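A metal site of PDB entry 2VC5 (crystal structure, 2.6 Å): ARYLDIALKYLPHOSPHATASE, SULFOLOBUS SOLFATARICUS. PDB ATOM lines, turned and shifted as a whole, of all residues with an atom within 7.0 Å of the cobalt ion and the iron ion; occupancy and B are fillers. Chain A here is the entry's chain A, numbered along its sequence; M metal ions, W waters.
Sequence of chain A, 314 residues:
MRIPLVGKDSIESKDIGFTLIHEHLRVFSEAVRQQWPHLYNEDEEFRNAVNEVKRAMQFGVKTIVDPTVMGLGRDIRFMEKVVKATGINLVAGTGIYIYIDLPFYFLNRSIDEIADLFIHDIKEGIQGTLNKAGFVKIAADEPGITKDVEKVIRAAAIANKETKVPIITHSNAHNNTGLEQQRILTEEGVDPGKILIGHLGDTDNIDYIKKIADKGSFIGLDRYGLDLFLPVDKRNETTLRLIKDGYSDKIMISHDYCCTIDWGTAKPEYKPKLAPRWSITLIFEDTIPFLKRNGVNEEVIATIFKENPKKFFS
The cobalt ion is bound by water W1 (1.8 Å), OQ1 of KCX 137 (2.0 Å), ND1 of His 170 (2.0 Å) and NE2 of His 199 (2.1 Å).
The cobalt ion has four donor atoms within binding distance.
SG of Cys 258 sits at hydrogen-bond distance from O of Asp 256 (3.6 Å).
A ring nitrogen (ND1) of His 199 lies within hydrogen-bond range of the guanidinium group of Arg 223.
The side-chain carboxylate (OE2) of Glu 23 sits at hydrogen-bond distance from the backbone NH (N) of Asp 256 (3.5 Å).
NE2 of His 170 lies within hydrogen-bond range of OD2 of Asp 141 (2.8 Å).
N of Asp 256 lies within hydrogen-bond range of O of Asp 222 (3.1 Å).
A ring nitrogen (ND1) of His 170 sits close to the side-chain hydroxyl (OH) of Tyr 97 (3.4 Å).
N of His 170 sits at hydrogen-bond distance from O of Ile 138.
ND1 of His 24 lies within hydrogen-bond range of OG1 of Thr 68 (2.7 Å).
Arg 223 touches the cobalt ion.
Within 4 Å of the cobalt ion: KCX 137, His 170, His 199 and Arg 223.
Water W1 binds the iron ion (2.0 Å).
OQ2 of KCX 137 is bound to the iron ion.
The iron ion is bound by OD2 of Asp 256 (2.1 Å).
NE2 of His 22 binds the iron ion (2.2 Å).
NE2 of His 24 binds the iron ion (2.2 Å).
Of the 23 residues printed, 4 come within 4 Å of the iron ion.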
ATOM      1  N   HIS A  22     -19.145   5.937 -18.460  1.00  0.00           N
ATOM      2  CA  HIS A  22     -18.964   7.199 -17.738  1.00  0.00           C
ATOM      3  C   HIS A  22     -19.999   8.240 -18.159  1.00  0.00           C
ATOM      4  O   HIS A  22     -19.758   9.018 -19.083  1.00  0.00           O
ATOM      5  CB  HIS A  22     -17.535   7.715 -17.954  1.00  0.00           C
ATOM      6  CG  HIS A  22     -17.096   8.725 -16.940  1.00  0.00           C
ATOM      7  ND1 HIS A  22     -15.977   8.545 -16.154  1.00  0.00           N
ATOM      8  CD2 HIS A  22     -17.609   9.932 -16.609  1.00  0.00           C
ATOM      9  CE1 HIS A  22     -15.824   9.602 -15.368  1.00  0.00           C
ATOM     10  NE2 HIS A  22     -16.798  10.460 -15.622  1.00  0.00           N
ATOM     11  N   GLU A  23     -21.132   8.252 -17.459  1.00  0.00           N
ATOM     12  CA  GLU A  23     -22.208   9.229 -17.705  1.00  0.00           C
ATOM     13  C   GLU A  23     -22.825   9.682 -16.385  1.00  0.00           C
ATOM     14  O   GLU A  23     -22.973   8.878 -15.470  1.00  0.00           O
ATOM     15  CB  GLU A  23     -23.317   8.626 -18.588  1.00  0.00           C
ATOM     16  CG  GLU A  23     -22.847   7.907 -19.862  1.00  0.00           C
ATOM     17  CD  GLU A  23     -22.239   8.825 -20.898  1.00  0.00           C
ATOM     18  OE1 GLU A  23     -21.475   8.330 -21.751  1.00  0.00           O
ATOM     19  OE2 GLU A  23     -22.510  10.048 -20.870  1.00  0.00           O
ATOM     20  N   HIS A  24     -23.194  10.953 -16.302  1.00  0.00           N
ATOM     21  CA  HIS A  24     -23.789  11.497 -15.078  1.00  0.00           C
ATOM     22  C   HIS A  24     -25.258  11.850 -15.289  1.00  0.00           C
ATOM     23  O   HIS A  24     -25.604  12.574 -16.236  1.00  0.00           O
ATOM     24  CB  HIS A  24     -23.024  12.736 -14.618  1.00  0.00           C
ATOM     25  CG  HIS A  24     -21.607  12.473 -14.214  1.00  0.00           C
ATOM     26  ND1 HIS A  24     -21.256  12.056 -12.955  1.00  0.00           N
ATOM     27  CD2 HIS A  24     -20.448  12.583 -14.911  1.00  0.00           C
ATOM     28  CE1 HIS A  24     -19.940  11.907 -12.886  1.00  0.00           C
ATOM     29  NE2 HIS A  24     -19.428  12.226 -14.066  1.00  0.00           N
ATOM     30  N   VAL A  27     -25.198  16.232 -11.660  1.00  0.00           N
ATOM     31  CA  VAL A  27     -24.184  16.621 -10.670  1.00  0.00           C
ATOM     32  C   VAL A  27     -24.506  17.985 -10.063  1.00  0.00           C
ATOM     33  O   VAL A  27     -25.086  18.849 -10.725  1.00  0.00           O
ATOM     34  CB  VAL A  27     -22.711  16.566 -11.218  1.00  0.00           C
ATOM     35  CG1 VAL A  27     -22.614  15.764 -12.500  1.00  0.00           C
ATOM     36  CG2 VAL A  27     -22.117  17.957 -11.416  1.00  0.00           C
ATOM     37  N   PRO A  67     -20.591   7.565 -12.292  1.00  0.00           N
ATOM     38  CA  PRO A  67     -19.539   7.822 -11.312  1.00  0.00           C
ATOM     39  C   PRO A  67     -19.717   9.113 -10.505  1.00  0.00           C
ATOM     40  O   PRO A  67     -18.730   9.705 -10.054  1.00  0.00           O
ATOM     41  CB  PRO A  67     -18.280   7.883 -12.183  1.00  0.00           C
ATOM     42  CG  PRO A  67     -18.756   8.346 -13.529  1.00  0.00           C
ATOM     43  CD  PRO A  67     -20.247   8.099 -13.620  1.00  0.00           C
ATOM     44  N   THR A  68     -20.959   9.533 -10.321  1.00  0.00           N
ATOM     45  CA  THR A  68     -21.298  10.626  -9.416  1.00  0.00           C
ATOM     46  C   THR A  68     -21.080  10.130  -7.982  1.00  0.00           C
ATOM     47  O   THR A  68     -21.760   9.214  -7.520  1.00  0.00           O
ATOM     48  CB  THR A  68     -22.761  11.087  -9.578  1.00  0.00           C
ATOM     49  OG1 THR A  68     -23.014  11.372 -10.969  1.00  0.00           O
ATOM     50  CG2 THR A  68     -23.029  12.335  -8.765  1.00  0.00           C
ATOM     51  N   LEU A  72     -19.787  15.479  -6.034  1.00  0.00           N
ATOM     52  CA  LEU A  72     -20.562  15.648  -7.264  1.00  0.00           C
ATOM     53  C   LEU A  72     -22.072  15.483  -7.049  1.00  0.00           C
ATOM     54  O   LEU A  72     -22.855  15.555  -8.000  1.00  0.00           O
ATOM     55  CB  LEU A  72     -20.072  14.681  -8.364  1.00  0.00           C
ATOM     56  CG  LEU A  72     -18.637  14.781  -8.893  1.00  0.00           C
ATOM     57  CD1 LEU A  72     -18.378  13.654  -9.882  1.00  0.00           C
ATOM     58  CD2 LEU A  72     -18.351  16.134  -9.549  1.00  0.00           C
ATOM     59  N   TYR A  97     -14.642  12.758  -4.782  1.00  0.00           N
ATOM     60  CA  TYR A  97     -14.212  13.593  -5.891  1.00  0.00           C
ATOM     61  C   TYR A  97     -13.623  14.906  -5.368  1.00  0.00           C
ATOM     62  O   TYR A  97     -14.358  15.810  -4.952  1.00  0.00           O
ATOM     63  CB  TYR A  97     -15.396  13.879  -6.819  1.00  0.00           C
ATOM     64  CG  TYR A  97     -15.040  14.575  -8.110  1.00  0.00           C
ATOM     65  CD1 TYR A  97     -14.958  15.966  -8.176  1.00  0.00           C
ATOM     66  CD2 TYR A  97     -14.798  13.841  -9.273  1.00  0.00           C
ATOM     67  CE1 TYR A  97     -14.632  16.616  -9.365  1.00  0.00           C
ATOM     68  CE2 TYR A  97     -14.480  14.480 -10.466  1.00  0.00           C
ATOM     69  CZ  TYR A  97     -14.396  15.858 -10.500  1.00  0.00           C
ATOM     70  OH  TYR A  97     -14.084  16.491 -11.689  1.00  0.00           O
ATOM     71  N   TYR A  99      -9.946  17.726  -5.965  1.00  0.00           N
ATOM     72  CA  TYR A  99      -8.716  18.070  -6.686  1.00  0.00           C
ATOM     73  C   TYR A  99      -7.584  18.463  -5.738  1.00  0.00           C
ATOM     74  O   TYR A  99      -6.411  18.307  -6.081  1.00  0.00           O
ATOM     75  CB  TYR A  99      -8.933  19.203  -7.690  1.00  0.00           C
ATOM     76  CG  TYR A  99      -9.885  18.932  -8.842  1.00  0.00           C
ATOM     77  CD1 TYR A  99     -10.332  17.643  -9.145  1.00  0.00           C
ATOM     78  CD2 TYR A  99     -10.320  19.984  -9.667  1.00  0.00           C
ATOM     79  CE1 TYR A  99     -11.211  17.416 -10.209  1.00  0.00           C
ATOM     80  CE2 TYR A  99     -11.185  19.763 -10.723  1.00  0.00           C
ATOM     81  CZ  TYR A  99     -11.630  18.479 -10.994  1.00  0.00           C
ATOM     82  OH  TYR A  99     -12.481  18.276 -12.049  1.00  0.00           O
ATOM     83  N   KCX A 137     -14.854   5.587  -7.257  1.00  0.00           N
ATOM     84  CA  KCX A 137     -14.398   6.707  -8.075  1.00  0.00           C
ATOM     85  CB  KCX A 137     -15.593   7.527  -8.575  1.00  0.00           C
ATOM     86  CG  KCX A 137     -15.395   8.181  -9.943  1.00  0.00           C
ATOM     87  CD  KCX A 137     -14.640   9.491  -9.876  1.00  0.00           C
ATOM     88  CE  KCX A 137     -14.499  10.115 -11.259  1.00  0.00           C
ATOM     89  NZ  KCX A 137     -15.787  10.691 -11.763  1.00  0.00           N
ATOM     90  C   KCX A 137     -13.435   7.610  -7.303  1.00  0.00           C
ATOM     91  O   KCX A 137     -13.727   8.038  -6.189  1.00  0.00           O
ATOM     92  CX  KCX A 137     -15.813  11.636 -12.707  1.00  0.00           C
ATOM     93  OQ1 KCX A 137     -14.775  12.072 -13.221  1.00  0.00           O
ATOM     94  OQ2 KCX A 137     -16.901  12.091 -13.089  1.00  0.00           O
ATOM     95  N   ILE A 138     -12.292   7.885  -7.929  1.00  0.00           N
ATOM     96  CA  ILE A 138     -11.296   8.826  -7.385  1.00  0.00           C
ATOM     97  C   ILE A 138     -10.912   9.861  -8.445  1.00  0.00           C
ATOM     98  O   ILE A 138     -11.209   9.681  -9.625  1.00  0.00           O
ATOM     99  CB  ILE A 138     -10.051   8.085  -6.807  1.00  0.00           C
ATOM    100  CG1 ILE A 138      -9.343   7.244  -7.874  1.00  0.00           C
ATOM    101  CG2 ILE A 138     -10.435   7.209  -5.635  1.00  0.00           C
ATOM    102  CD1 ILE A 138      -8.061   7.847  -8.371  1.00  0.00           C
ATOM    103  N   ALA A 139     -10.272  10.948  -8.025  1.00  0.00           N
ATOM    104  CA  ALA A 139      -9.989  12.073  -8.927  1.00  0.00           C
ATOM    105  C   ALA A 139      -8.638  12.756  -8.689  1.00  0.00           C
ATOM    106  O   ALA A 139      -8.076  12.679  -7.598  1.00  0.00           O
ATOM    107  CB  ALA A 139     -11.124  13.083  -8.859  1.00  0.00           C
ATOM    108  N   ASP A 141      -6.470  16.444 -10.708  1.00  0.00           N
ATOM    109  CA  ASP A 141      -6.467  17.401 -11.804  1.00  0.00           C
ATOM    110  C   ASP A 141      -5.174  18.238 -11.869  1.00  0.00           C
ATOM    111  O   ASP A 141      -4.107  17.743 -11.508  1.00  0.00           O
ATOM    112  CB  ASP A 141      -7.719  18.282 -11.756  1.00  0.00           C
ATOM    113  CG  ASP A 141      -8.325  18.524 -13.134  1.00  0.00           C
ATOM    114  OD1 ASP A 141      -7.667  19.153 -13.981  1.00  0.00           O
ATOM    115  OD2 ASP A 141      -9.463  18.065 -13.369  1.00  0.00           O
ATOM    116  N   THR A 169     -11.311   6.439 -12.494  1.00  0.00           N
ATOM    117  CA  THR A 169     -10.599   7.663 -12.142  1.00  0.00           C
ATOM    118  C   THR A 169     -11.004   8.845 -13.018  1.00  0.00           C
ATOM    119  O   THR A 169     -11.406   8.673 -14.164  1.00  0.00           O
ATOM    120  CB  THR A 169      -9.070   7.507 -12.242  1.00  0.00           C
ATOM    121  OG1 THR A 169      -8.666   7.565 -13.618  1.00  0.00           O
ATOM    122  CG2 THR A 169      -8.601   6.191 -11.627  1.00  0.00           C
ATOM    123  N   HIS A 170     -10.884  10.030 -12.435  1.00  0.00           N
ATOM    124  CA  HIS A 170     -10.867  11.286 -13.165  1.00  0.00           C
ATOM    125  C   HIS A 170      -9.398  11.726 -13.141  1.00  0.00           C
ATOM    126  O   HIS A 170      -8.738  11.619 -12.104  1.00  0.00           O
ATOM    127  CB  HIS A 170     -11.750  12.309 -12.453  1.00  0.00           C
ATOM    128  CG  HIS A 170     -11.601  13.717 -12.963  1.00  0.00           C
ATOM    129  ND1 HIS A 170     -12.561  14.328 -13.750  1.00  0.00           N
ATOM    130  CD2 HIS A 170     -10.626  14.636 -12.776  1.00  0.00           C
ATOM    131  CE1 HIS A 170     -12.171  15.561 -14.030  1.00  0.00           C
ATOM    132  NE2 HIS A 170     -11.000  15.772 -13.454  1.00  0.00           N
ATOM    133  N   SER A 171      -8.895  12.205 -14.269  1.00  0.00           N
ATOM    134  CA  SER A 171      -7.532  12.748 -14.335  1.00  0.00           C
ATOM    135  C   SER A 171      -7.416  13.895 -15.331  1.00  0.00           C
ATOM    136  O   SER A 171      -8.276  14.061 -16.198  1.00  0.00           O
ATOM    137  CB  SER A 171      -6.511  11.658 -14.658  1.00  0.00           C
ATOM    138  OG  SER A 171      -6.260  11.579 -16.049  1.00  0.00           O
ATOM    139  N   GLY A 198      -9.312   7.789 -16.360  1.00  0.00           N
ATOM    140  CA  GLY A 198     -10.274   8.633 -17.049  1.00  0.00           C
ATOM    141  C   GLY A 198      -9.704   9.823 -17.796  1.00  0.00           C
ATOM    142  O   GLY A 198      -8.628  10.324 -17.479  1.00  0.00           O
ATOM    143  N   HIS A 199     -10.463  10.256 -18.805  1.00  0.00           N
ATOM    144  CA  HIS A 199     -10.233  11.512 -19.528  1.00  0.00           C
ATOM    145  C   HIS A 199      -8.936  11.572 -20.339  1.00  0.00           C
ATOM    146  O   HIS A 199      -8.394  12.651 -20.595  1.00  0.00           O
ATOM    147  CB  HIS A 199     -10.390  12.718 -18.594  1.00  0.00           C
ATOM    148  CG  HIS A 199     -11.592  12.635 -17.710  1.00  0.00           C
ATOM    149  ND1 HIS A 199     -12.841  12.298 -18.190  1.00  0.00           N
ATOM    150  CD2 HIS A 199     -11.749  12.828 -16.385  1.00  0.00           C
ATOM    151  CE1 HIS A 199     -13.707  12.294 -17.198  1.00  0.00           C
ATOM    152  NE2 HIS A 199     -13.070  12.606 -16.089  1.00  0.00           N
ATOM    153  N   ASP A 222     -13.352   9.162 -22.915  1.00  0.00           N
ATOM    154  CA  ASP A 222     -14.672   9.172 -22.281  1.00  0.00           C
ATOM    155  C   ASP A 222     -15.398  10.522 -22.230  1.00  0.00           C
ATOM    156  O   ASP A 222     -16.407  10.658 -21.531  1.00  0.00           O
ATOM    157  CB  ASP A 222     -14.544   8.605 -20.858  1.00  0.00           C
ATOM    158  CG  ASP A 222     -13.446   9.274 -20.042  1.00  0.00           C
ATOM    159  OD1 ASP A 222     -12.843   8.588 -19.199  1.00  0.00           O
ATOM    160  OD2 ASP A 222     -13.167  10.473 -20.262  1.00  0.00           O
ATOM    161  N   ARG A 223     -14.915  11.513 -22.977  1.00  0.00           N
ATOM    162  CA  ARG A 223     -15.515  12.850 -22.956  1.00  0.00           C
ATOM    163  C   ARG A 223     -15.972  13.355 -24.331  1.00  0.00           C
ATOM    164  O   ARG A 223     -15.879  14.552 -24.617  1.00  0.00           O
ATOM    165  CB  ARG A 223     -14.566  13.856 -22.298  1.00  0.00           C
ATOM    166  CG  ARG A 223     -14.583  13.826 -20.782  1.00  0.00           C
ATOM    167  CD  ARG A 223     -13.724  14.924 -20.207  1.00  0.00           C
ATOM    168  NE  ARG A 223     -14.073  15.208 -18.818  1.00  0.00           N
ATOM    169  CZ  ARG A 223     -13.434  16.069 -18.034  1.00  0.00           C
ATOM    170  NH1 ARG A 223     -13.835  16.264 -16.789  1.00  0.00           N
ATOM    171  NH2 ARG A 223     -12.394  16.746 -18.503  1.00  0.00           N
ATOM    172  N   ASP A 256     -19.274  11.358 -20.716  1.00  0.00           N
ATOM    173  CA  ASP A 256     -19.161  12.156 -19.483  1.00  0.00           C
ATOM    174  C   ASP A 256     -20.289  13.201 -19.427  1.00  0.00           C
ATOM    175  O   ASP A 256     -20.181  14.202 -18.723  1.00  0.00           O
ATOM    176  CB  ASP A 256     -17.778  12.803 -19.366  1.00  0.00           C
ATOM    177  CG  ASP A 256     -17.466  13.317 -17.963  1.00  0.00           C
ATOM    178  OD1 ASP A 256     -16.533  14.132 -17.827  1.00  0.00           O
ATOM    179  OD2 ASP A 256     -18.147  12.908 -16.997  1.00  0.00           O
ATOM    180  N   TYR A 257     -21.360  12.947 -20.169  1.00  0.00           N
ATOM    181  CA  TYR A 257     -22.477  13.876 -20.239  1.00  0.00           C
ATOM    182  C   TYR A 257     -23.220  13.991 -18.921  1.00  0.00           C
ATOM    183  O   TYR A 257     -23.508  12.990 -18.257  1.00  0.00           O
ATOM    184  CB  TYR A 257     -23.454  13.533 -21.368  1.00  0.00           C
ATOM    185  CG  TYR A 257     -24.537  14.588 -21.558  1.00  0.00           C
ATOM    186  CD1 TYR A 257     -24.245  15.801 -22.171  1.00  0.00           C
ATOM    187  CD2 TYR A 257     -25.837  14.368 -21.108  1.00  0.00           C
ATOM    188  CE1 TYR A 257     -25.225  16.777 -22.335  1.00  0.00           C
ATOM    189  CE2 TYR A 257     -26.824  15.338 -21.268  1.00  0.00           C
ATOM    190  CZ  TYR A 257     -26.511  16.540 -21.886  1.00  0.00           C
ATOM    191  OH  TYR A 257     -27.483  17.498 -22.039  1.00  0.00           O
ATOM    192  N   CYS A 258     -23.513  15.230 -18.544  1.00  0.00           N
ATOM    193  CA  CYS A 258     -24.366  15.499 -17.397  1.00  0.00           C
ATOM    194  C   CYS A 258     -25.648  16.116 -17.904  1.00  0.00           C
ATOM    195  O   CYS A 258     -25.624  17.146 -18.594  1.00  0.00           O
ATOM    196  CB  CYS A 258     -23.672  16.447 -16.420  1.00  0.00           C
ATOM    197  SG  CYS A 258     -21.900  16.153 -16.207  1.00  0.00           S
HETATM  198 CO    CO M   1     -14.227  13.455 -14.562  1.00  0.00          CO
HETATM  199 FE    FE M   2     -17.455  12.474 -15.016  1.00  0.00          FE
HETATM  200  O   HOH W   1     -15.864  13.595 -15.239  1.00  0.00           O
